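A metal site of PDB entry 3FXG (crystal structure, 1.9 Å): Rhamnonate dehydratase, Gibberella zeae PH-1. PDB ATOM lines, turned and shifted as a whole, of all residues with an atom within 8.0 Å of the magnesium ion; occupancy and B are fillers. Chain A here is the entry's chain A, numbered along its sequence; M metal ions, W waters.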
ATOM      1  N   ARG A  56      18.831  -1.431  10.922  1.00  0.00           N
ATOM      2  CA  ARG A  56      18.332  -1.843   9.607  1.00  0.00           C
ATOM      3  C   ARG A  56      18.527  -3.341   9.423  1.00  0.00           C
ATOM      4  O   ARG A  56      17.846  -3.971   8.610  1.00  0.00           O
ATOM      5  CB  ARG A  56      19.017  -1.058   8.486  1.00  0.00           C
ATOM      6  CG  ARG A  56      18.623   0.425   8.481  1.00  0.00           C
ATOM      7  CD  ARG A  56      18.581   1.047   7.090  1.00  0.00           C
ATOM      8  NE  ARG A  56      19.906   1.362   6.564  1.00  0.00           N
ATOM      9  CZ  ARG A  56      20.120   1.976   5.414  1.00  0.00           C
ATOM     10  NH1 ARG A  56      19.105   2.344   4.642  1.00  0.00           N
ATOM     11  NH2 ARG A  56      21.361   2.240   5.012  1.00  0.00           N
ATOM     12  N   TYR A 167      29.726  13.211  -5.108  1.00  0.00           N
ATOM     13  CA  TYR A 167      29.092  13.842  -3.975  1.00  0.00           C
ATOM     14  C   TYR A 167      29.179  12.692  -2.963  1.00  0.00           C
ATOM     15  O   TYR A 167      29.251  11.531  -3.360  1.00  0.00           O
ATOM     16  CB  TYR A 167      27.649  14.277  -4.268  1.00  0.00           C
ATOM     17  CG  TYR A 167      26.632  13.169  -4.471  1.00  0.00           C
ATOM     18  CD1 TYR A 167      26.018  12.555  -3.373  1.00  0.00           C
ATOM     19  CD2 TYR A 167      26.228  12.796  -5.754  1.00  0.00           C
ATOM     20  CE1 TYR A 167      25.032  11.594  -3.555  1.00  0.00           C
ATOM     21  CE2 TYR A 167      25.242  11.842  -5.943  1.00  0.00           C
ATOM     22  CZ  TYR A 167      24.636  11.247  -4.838  1.00  0.00           C
ATOM     23  OH  TYR A 167      23.645  10.309  -5.025  1.00  0.00           O
ATOM     24  N   THR A 169      27.677  10.432   0.191  1.00  0.00           N
ATOM     25  CA  THR A 169      26.497  10.032   0.958  1.00  0.00           C
ATOM     26  C   THR A 169      26.961   9.506   2.313  1.00  0.00           C
ATOM     27  O   THR A 169      27.727   8.553   2.397  1.00  0.00           O
ATOM     28  CB  THR A 169      25.698   8.924   0.251  1.00  0.00           C
ATOM     29  OG1 THR A 169      25.311   9.383  -1.051  1.00  0.00           O
ATOM     30  CG2 THR A 169      24.451   8.561   1.048  1.00  0.00           C
ATOM     31  N   LYS A 185      25.096  14.059   0.900  1.00  0.00           N
ATOM     32  CA  LYS A 185      23.723  13.547   1.030  1.00  0.00           C
ATOM     33  C   LYS A 185      23.590  12.816   2.368  1.00  0.00           C
ATOM     34  O   LYS A 185      24.305  11.847   2.629  1.00  0.00           O
ATOM     35  CB  LYS A 185      23.388  12.584  -0.111  1.00  0.00           C
ATOM     36  CG  LYS A 185      21.918  12.144  -0.131  1.00  0.00           C
ATOM     37  CD  LYS A 185      21.557  11.364  -1.403  1.00  0.00           C
ATOM     38  CE  LYS A 185      22.284  10.034  -1.471  1.00  0.00           C
ATOM     39  NZ  LYS A 185      21.994   9.305  -2.742  1.00  0.00           N
ATOM     40  N   VAL A 221      19.044  15.026   0.632  1.00  0.00           N
ATOM     41  CA  VAL A 221      18.470  14.197   1.691  1.00  0.00           C
ATOM     42  C   VAL A 221      17.953  12.871   1.161  1.00  0.00           C
ATOM     43  O   VAL A 221      17.103  12.835   0.271  1.00  0.00           O
ATOM     44  CB  VAL A 221      17.302  14.943   2.394  1.00  0.00           C
ATOM     45  CG1 VAL A 221      16.768  14.104   3.545  1.00  0.00           C
ATOM     46  CG2 VAL A 221      17.794  16.306   2.902  1.00  0.00           C
ATOM     47  N   ASP A 222      18.458  11.776   1.715  1.00  0.00           N
ATOM     48  CA  ASP A 222      18.027  10.440   1.296  1.00  0.00           C
ATOM     49  C   ASP A 222      16.929   9.974   2.230  1.00  0.00           C
ATOM     50  O   ASP A 222      17.095   9.990   3.448  1.00  0.00           O
ATOM     51  CB  ASP A 222      19.198   9.469   1.343  1.00  0.00           C
ATOM     52  CG  ASP A 222      18.892   8.152   0.645  1.00  0.00           C
ATOM     53  OD1 ASP A 222      17.967   7.440   1.083  1.00  0.00           O
ATOM     54  OD2 ASP A 222      19.575   7.842  -0.348  1.00  0.00           O
ATOM     55  N   CYS A 223      15.803   9.551   1.667  1.00  0.00           N
ATOM     56  CA  CYS A 223      14.662   9.118   2.459  1.00  0.00           C
ATOM     57  C   CYS A 223      14.381   7.610   2.421  1.00  0.00           C
ATOM     58  O   CYS A 223      13.398   7.144   3.011  1.00  0.00           O
ATOM     59  CB  CYS A 223      13.419   9.901   2.036  1.00  0.00           C
ATOM     60  SG  CYS A 223      13.612  11.714   2.201  1.00  0.00           S
ATOM     61  N   TYR A 224      15.241   6.860   1.740  1.00  0.00           N
ATOM     62  CA  TYR A 224      15.134   5.407   1.630  1.00  0.00           C
ATOM     63  C   TYR A 224      13.688   4.861   1.536  1.00  0.00           C
ATOM     64  O   TYR A 224      13.258   4.085   2.393  1.00  0.00           O
ATOM     65  CB  TYR A 224      15.871   4.752   2.812  1.00  0.00           C
ATOM     66  CG  TYR A 224      16.201   3.284   2.615  1.00  0.00           C
ATOM     67  CD1 TYR A 224      17.060   2.867   1.601  1.00  0.00           C
ATOM     68  CD2 TYR A 224      15.621   2.303   3.437  1.00  0.00           C
ATOM     69  CE1 TYR A 224      17.352   1.508   1.409  1.00  0.00           C
ATOM     70  CE2 TYR A 224      15.903   0.947   3.247  1.00  0.00           C
ATOM     71  CZ  TYR A 224      16.762   0.559   2.235  1.00  0.00           C
ATOM     72  OH  TYR A 224      17.014  -0.780   2.031  1.00  0.00           O
ATOM     73  N   MET A 225      12.978   5.273   0.483  1.00  0.00           N
ATOM     74  CA  MET A 225      11.589   4.860   0.215  1.00  0.00           C
ATOM     75  C   MET A 225      10.685   4.749   1.448  1.00  0.00           C
ATOM     76  O   MET A 225       9.756   3.946   1.484  1.00  0.00           O
ATOM     77  CB  MET A 225      11.594   3.532  -0.566  1.00  0.00           C
ATOM     78  CG  MET A 225      12.271   2.341   0.122  1.00  0.00           C
ATOM     79  SD  MET A 225      12.619   0.776  -1.032  1.00  0.00           S
ATOM     80  CE  MET A 225      14.118   0.053  -0.047  1.00  0.00           C
ATOM     81  N   TRP A 246      18.256  18.340  -3.295  1.00  0.00           N
ATOM     82  CA  TRP A 246      17.244  17.416  -3.782  1.00  0.00           C
ATOM     83  C   TRP A 246      16.849  16.404  -2.718  1.00  0.00           C
ATOM     84  O   TRP A 246      17.607  16.129  -1.793  1.00  0.00           O
ATOM     85  CB  TRP A 246      17.685  16.700  -5.072  1.00  0.00           C
ATOM     86  CG  TRP A 246      18.619  15.518  -4.918  1.00  0.00           C
ATOM     87  CD1 TRP A 246      18.367  14.339  -4.261  1.00  0.00           C
ATOM     88  CD2 TRP A 246      19.920  15.372  -5.509  1.00  0.00           C
ATOM     89  NE1 TRP A 246      19.432  13.479  -4.411  1.00  0.00           N
ATOM     90  CE2 TRP A 246      20.390  14.083  -5.164  1.00  0.00           C
ATOM     91  CE3 TRP A 246      20.733  16.207  -6.286  1.00  0.00           C
ATOM     92  CZ2 TRP A 246      21.647  13.614  -5.586  1.00  0.00           C
ATOM     93  CZ3 TRP A 246      21.980  15.734  -6.698  1.00  0.00           C
ATOM     94  CH2 TRP A 246      22.418  14.447  -6.354  1.00  0.00           C
ATOM     95  N   GLU A 248      15.733  12.575  -2.101  1.00  0.00           N
ATOM     96  CA  GLU A 248      15.855  11.259  -2.718  1.00  0.00           C
ATOM     97  C   GLU A 248      14.977  10.126  -2.185  1.00  0.00           C
ATOM     98  O   GLU A 248      14.843   9.926  -0.985  1.00  0.00           O
ATOM     99  CB  GLU A 248      17.324  10.839  -2.662  1.00  0.00           C
ATOM    100  CG  GLU A 248      17.654   9.572  -3.423  1.00  0.00           C
ATOM    101  CD  GLU A 248      19.145   9.391  -3.608  1.00  0.00           C
ATOM    102  OE1 GLU A 248      19.832  10.390  -3.895  1.00  0.00           O
ATOM    103  OE2 GLU A 248      19.635   8.245  -3.472  1.00  0.00           O
ATOM    104  N   GLU A 249      14.399   9.379  -3.135  1.00  0.00           N
ATOM    105  CA  GLU A 249      13.535   8.228  -2.844  1.00  0.00           C
ATOM    106  C   GLU A 249      12.565   8.470  -1.691  1.00  0.00           C
ATOM    107  O   GLU A 249      12.500   7.669  -0.755  1.00  0.00           O
ATOM    108  CB  GLU A 249      14.389   6.985  -2.574  1.00  0.00           C
ATOM    109  CG  GLU A 249      13.715   5.695  -3.040  1.00  0.00           C
ATOM    110  CD  GLU A 249      14.577   4.447  -2.872  1.00  0.00           C
ATOM    111  OE1 GLU A 249      14.203   3.400  -3.451  1.00  0.00           O
ATOM    112  OE2 GLU A 249      15.618   4.507  -2.168  1.00  0.00           O
ATOM    113  N   THR A 272      14.345  12.865  -6.641  1.00  0.00           N
ATOM    114  CA  THR A 272      15.017  11.794  -7.359  1.00  0.00           C
ATOM    115  C   THR A 272      14.588  10.438  -6.809  1.00  0.00           C
ATOM    116  O   THR A 272      13.992  10.359  -5.728  1.00  0.00           O
ATOM    117  CB  THR A 272      16.552  11.883  -7.216  1.00  0.00           C
ATOM    118  OG1 THR A 272      16.947  11.444  -5.907  1.00  0.00           O
ATOM    119  CG2 THR A 272      17.027  13.330  -7.417  1.00  0.00           C
ATOM    120  N   THR A 273      14.883   9.376  -7.540  1.00  0.00           N
ATOM    121  CA  THR A 273      14.553   8.022  -7.120  1.00  0.00           C
ATOM    122  C   THR A 273      15.028   7.043  -8.175  1.00  0.00           C
ATOM    123  O   THR A 273      15.591   7.445  -9.192  1.00  0.00           O
ATOM    124  CB  THR A 273      13.023   7.837  -6.920  1.00  0.00           C
ATOM    125  OG1 THR A 273      12.758   6.564  -6.330  1.00  0.00           O
ATOM    126  CG2 THR A 273      12.298   7.912  -8.266  1.00  0.00           C
ATOM    127  N   GLY A 274      14.832   5.754  -7.919  1.00  0.00           N
ATOM    128  CA  GLY A 274      15.208   4.748  -8.896  1.00  0.00           C
ATOM    129  C   GLY A 274      16.130   3.620  -8.491  1.00  0.00           C
ATOM    130  O   GLY A 274      16.236   2.633  -9.221  1.00  0.00           O
ATOM    131  N   GLU A 275      16.808   3.710  -7.352  1.00  0.00           N
ATOM    132  CA  GLU A 275      17.716   2.631  -6.985  1.00  0.00           C
ATOM    133  C   GLU A 275      17.000   1.305  -6.784  1.00  0.00           C
ATOM    134  O   GLU A 275      17.616   0.247  -6.875  1.00  0.00           O
ATOM    135  CB  GLU A 275      18.557   2.998  -5.754  1.00  0.00           C
ATOM    136  CG  GLU A 275      17.802   3.168  -4.454  1.00  0.00           C
ATOM    137  CD  GLU A 275      18.692   3.798  -3.382  1.00  0.00           C
ATOM    138  OE1 GLU A 275      18.850   3.183  -2.298  1.00  0.00           O
ATOM    139  OE2 GLU A 275      19.234   4.888  -3.634  1.00  0.00           O
ATOM    140  N   HIS A 276      15.694   1.347  -6.537  1.00  0.00           N
ATOM    141  CA  HIS A 276      14.947   0.112  -6.362  1.00  0.00           C
ATOM    142  C   HIS A 276      13.944  -0.127  -7.495  1.00  0.00           C
ATOM    143  O   HIS A 276      12.887  -0.722  -7.278  1.00  0.00           O
ATOM    144  CB  HIS A 276      14.253   0.093  -5.004  1.00  0.00           C
ATOM    145  CG  HIS A 276      15.219   0.107  -3.858  1.00  0.00           C
ATOM    146  ND1 HIS A 276      15.523   1.246  -3.152  1.00  0.00           N
ATOM    147  CD2 HIS A 276      15.990  -0.873  -3.334  1.00  0.00           C
ATOM    148  CE1 HIS A 276      16.440   0.973  -2.239  1.00  0.00           C
ATOM    149  NE2 HIS A 276      16.746  -0.307  -2.337  1.00  0.00           N
ATOM    150  N   GLN A 296      18.065   7.212 -10.554  1.00  0.00           N
ATOM    151  CA  GLN A 296      19.240   6.596  -9.957  1.00  0.00           C
ATOM    152  C   GLN A 296      19.265   5.076  -9.866  1.00  0.00           C
ATOM    153  O   GLN A 296      19.172   4.512  -8.770  1.00  0.00           O
ATOM    154  CB  GLN A 296      19.428   7.189  -8.561  1.00  0.00           C
ATOM    155  CG  GLN A 296      19.375   8.719  -8.558  1.00  0.00           C
ATOM    156  CD  GLN A 296      19.151   9.302  -7.167  1.00  0.00           C
ATOM    157  OE1 GLN A 296      18.135   9.033  -6.525  1.00  0.00           O
ATOM    158  NE2 GLN A 296      20.105  10.103  -6.710  1.00  0.00           N
ATOM    159  N   TRP A 301      21.720  -4.033  -9.828  1.00  0.00           N
ATOM    160  CA  TRP A 301      20.356  -4.461  -9.545  1.00  0.00           C
ATOM    161  C   TRP A 301      19.342  -4.356 -10.690  1.00  0.00           C
ATOM    162  O   TRP A 301      18.541  -5.265 -10.888  1.00  0.00           O
ATOM    163  CB  TRP A 301      19.785  -3.678  -8.354  1.00  0.00           C
ATOM    164  CG  TRP A 301      20.650  -3.651  -7.106  1.00  0.00           C
ATOM    165  CD1 TRP A 301      21.719  -4.442  -6.819  1.00  0.00           C
ATOM    166  CD2 TRP A 301      20.465  -2.806  -5.959  1.00  0.00           C
ATOM    167  NE1 TRP A 301      22.218  -4.145  -5.575  1.00  0.00           N
ATOM    168  CE2 TRP A 301      21.465  -3.142  -5.016  1.00  0.00           C
ATOM    169  CE3 TRP A 301      19.558  -1.782  -5.634  1.00  0.00           C
ATOM    170  CZ2 TRP A 301      21.590  -2.503  -3.778  1.00  0.00           C
ATOM    171  CZ3 TRP A 301      19.670  -1.147  -4.400  1.00  0.00           C
ATOM    172  CH2 TRP A 301      20.687  -1.512  -3.484  1.00  0.00           C
ATOM    173  N   HIS A 325      23.156   4.581  -8.381  1.00  0.00           N
ATOM    174  CA  HIS A 325      23.347   4.424  -6.952  1.00  0.00           C
ATOM    175  C   HIS A 325      24.642   3.688  -6.646  1.00  0.00           C
ATOM    176  O   HIS A 325      24.788   2.513  -6.980  1.00  0.00           O
ATOM    177  CB  HIS A 325      22.149   3.662  -6.363  1.00  0.00           C
ATOM    178  CG  HIS A 325      22.360   3.157  -4.967  1.00  0.00           C
ATOM    179  ND1 HIS A 325      23.060   2.001  -4.696  1.00  0.00           N
ATOM    180  CD2 HIS A 325      21.966   3.655  -3.775  1.00  0.00           C
ATOM    181  CE1 HIS A 325      23.090   1.803  -3.393  1.00  0.00           C
ATOM    182  NE2 HIS A 325      22.434   2.790  -2.812  1.00  0.00           N
ATOM    183  N   ALA A 326      25.593   4.390  -6.019  1.00  0.00           N
ATOM    184  CA  ALA A 326      26.896   3.832  -5.650  1.00  0.00           C
ATOM    185  C   ALA A 326      27.463   3.006  -6.798  1.00  0.00           C
ATOM    186  O   ALA A 326      27.820   3.555  -7.844  1.00  0.00           O
ATOM    187  CB  ALA A 326      26.756   2.974  -4.396  1.00  0.00           C
ATOM    188  N   GLU A 345      27.864   9.106  -7.260  1.00  0.00           N
ATOM    189  CA  GLU A 345      27.667   9.014  -5.831  1.00  0.00           C
ATOM    190  C   GLU A 345      28.698   8.080  -5.224  1.00  0.00           C
ATOM    191  O   GLU A 345      29.111   7.102  -5.846  1.00  0.00           O
ATOM    192  CB  GLU A 345      26.283   8.459  -5.505  1.00  0.00           C
ATOM    193  CG  GLU A 345      26.164   7.971  -4.067  1.00  0.00           C
ATOM    194  CD  GLU A 345      24.827   7.328  -3.740  1.00  0.00           C
ATOM    195  OE1 GLU A 345      24.327   6.536  -4.570  1.00  0.00           O
ATOM    196  OE2 GLU A 345      24.282   7.596  -2.648  1.00  0.00           O
ATOM    197  N   LEU A 347      29.088   6.161  -1.573  1.00  0.00           N
ATOM    198  CA  LEU A 347      28.483   5.868  -0.282  1.00  0.00           C
ATOM    199  C   LEU A 347      29.597   5.698   0.738  1.00  0.00           C
ATOM    200  O   LEU A 347      30.319   4.696   0.699  1.00  0.00           O
ATOM    201  CB  LEU A 347      27.635   4.590  -0.398  1.00  0.00           C
ATOM    202  CG  LEU A 347      26.714   4.185   0.754  1.00  0.00           C
ATOM    203  CD1 LEU A 347      25.846   3.009   0.312  1.00  0.00           C
ATOM    204  CD2 LEU A 347      27.530   3.811   1.981  1.00  0.00           C
HETATM  205 MG    MG M   1      19.560   6.480  -2.110  1.00  0.00          MG
HETATM  206  O   HOH W   1      17.724   5.703  -1.001  1.00  0.00           O
HETATM  207  O   HOH W   2      20.589   4.384  -0.581  1.00  0.00           O
HETATM  208  O   HOH W   3      22.042   6.349  -2.029  1.00  0.00           O
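The side-chain carboxylate (OD1) of Asp 222 lies within hydrogen-bond range of the backbone NH (N) of Tyr 224, at 2.9 Å.
OE1 of Glu 248 lies within salt-bridge range of NZ of Lys 185 (2.7 Å).
The backbone carbonyl oxygen of Val 221 sits at hydrogen-bond distance from the backbone NH of Glu 248 (2.8 Å).
NZ of Lys 185 sits at hydrogen-bond distance from OH of Tyr 167, at 3.0 Å.
The side-chain amino group of Lys 185 lies close to the side-chain carboxylate of Asp 222 (3.7 Å).
The side-chain carboxylate of Glu 345 is in salt-bridge range of the side-chain amino group of Lys 185, 2.9 Å away.
NE2 of Gln 296 is in hydrogen-bond range of OE1 of Glu 248 (2.8 Å).
The indole nitrogen (NE1) of Trp 246 lies within hydrogen-bond range of the side-chain carboxylate (OE1) of Glu 248 (3.2 Å).
Water W3 lies within hydrogen-bond range of OE2 of Glu 345 (2.6 Å) and NZ of Lys 185 (3.0 Å).
Water W2 bridges OE1 of Glu 275 and NE2 of His 325.
OD2 of Asp 222 is bound to the magnesium ion, at 2.2 Å.
OE2 of Glu 275 binds the magnesium ion, at 2.2 Å.
The side-chain carboxylate (OE2) of Glu 248 binds the magnesium ion, 2.2 Å away.
Water W1 is bound to the magnesium ion, at 2.3 Å.
The magnesium ion is bound by water W3, 2.5 Å away.
Slightly farther from the magnesium ion lies water W2 (2.8 Å).
Merely in contact with the magnesium ion: Lys 185 (3.8 Å).
Within 4 Å of the magnesium ion: Lys 185, Asp 222, Glu 248 and Glu 275.
The nearest printed residue that does not touch the magnesium ion is His 325 (4.1 Å).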
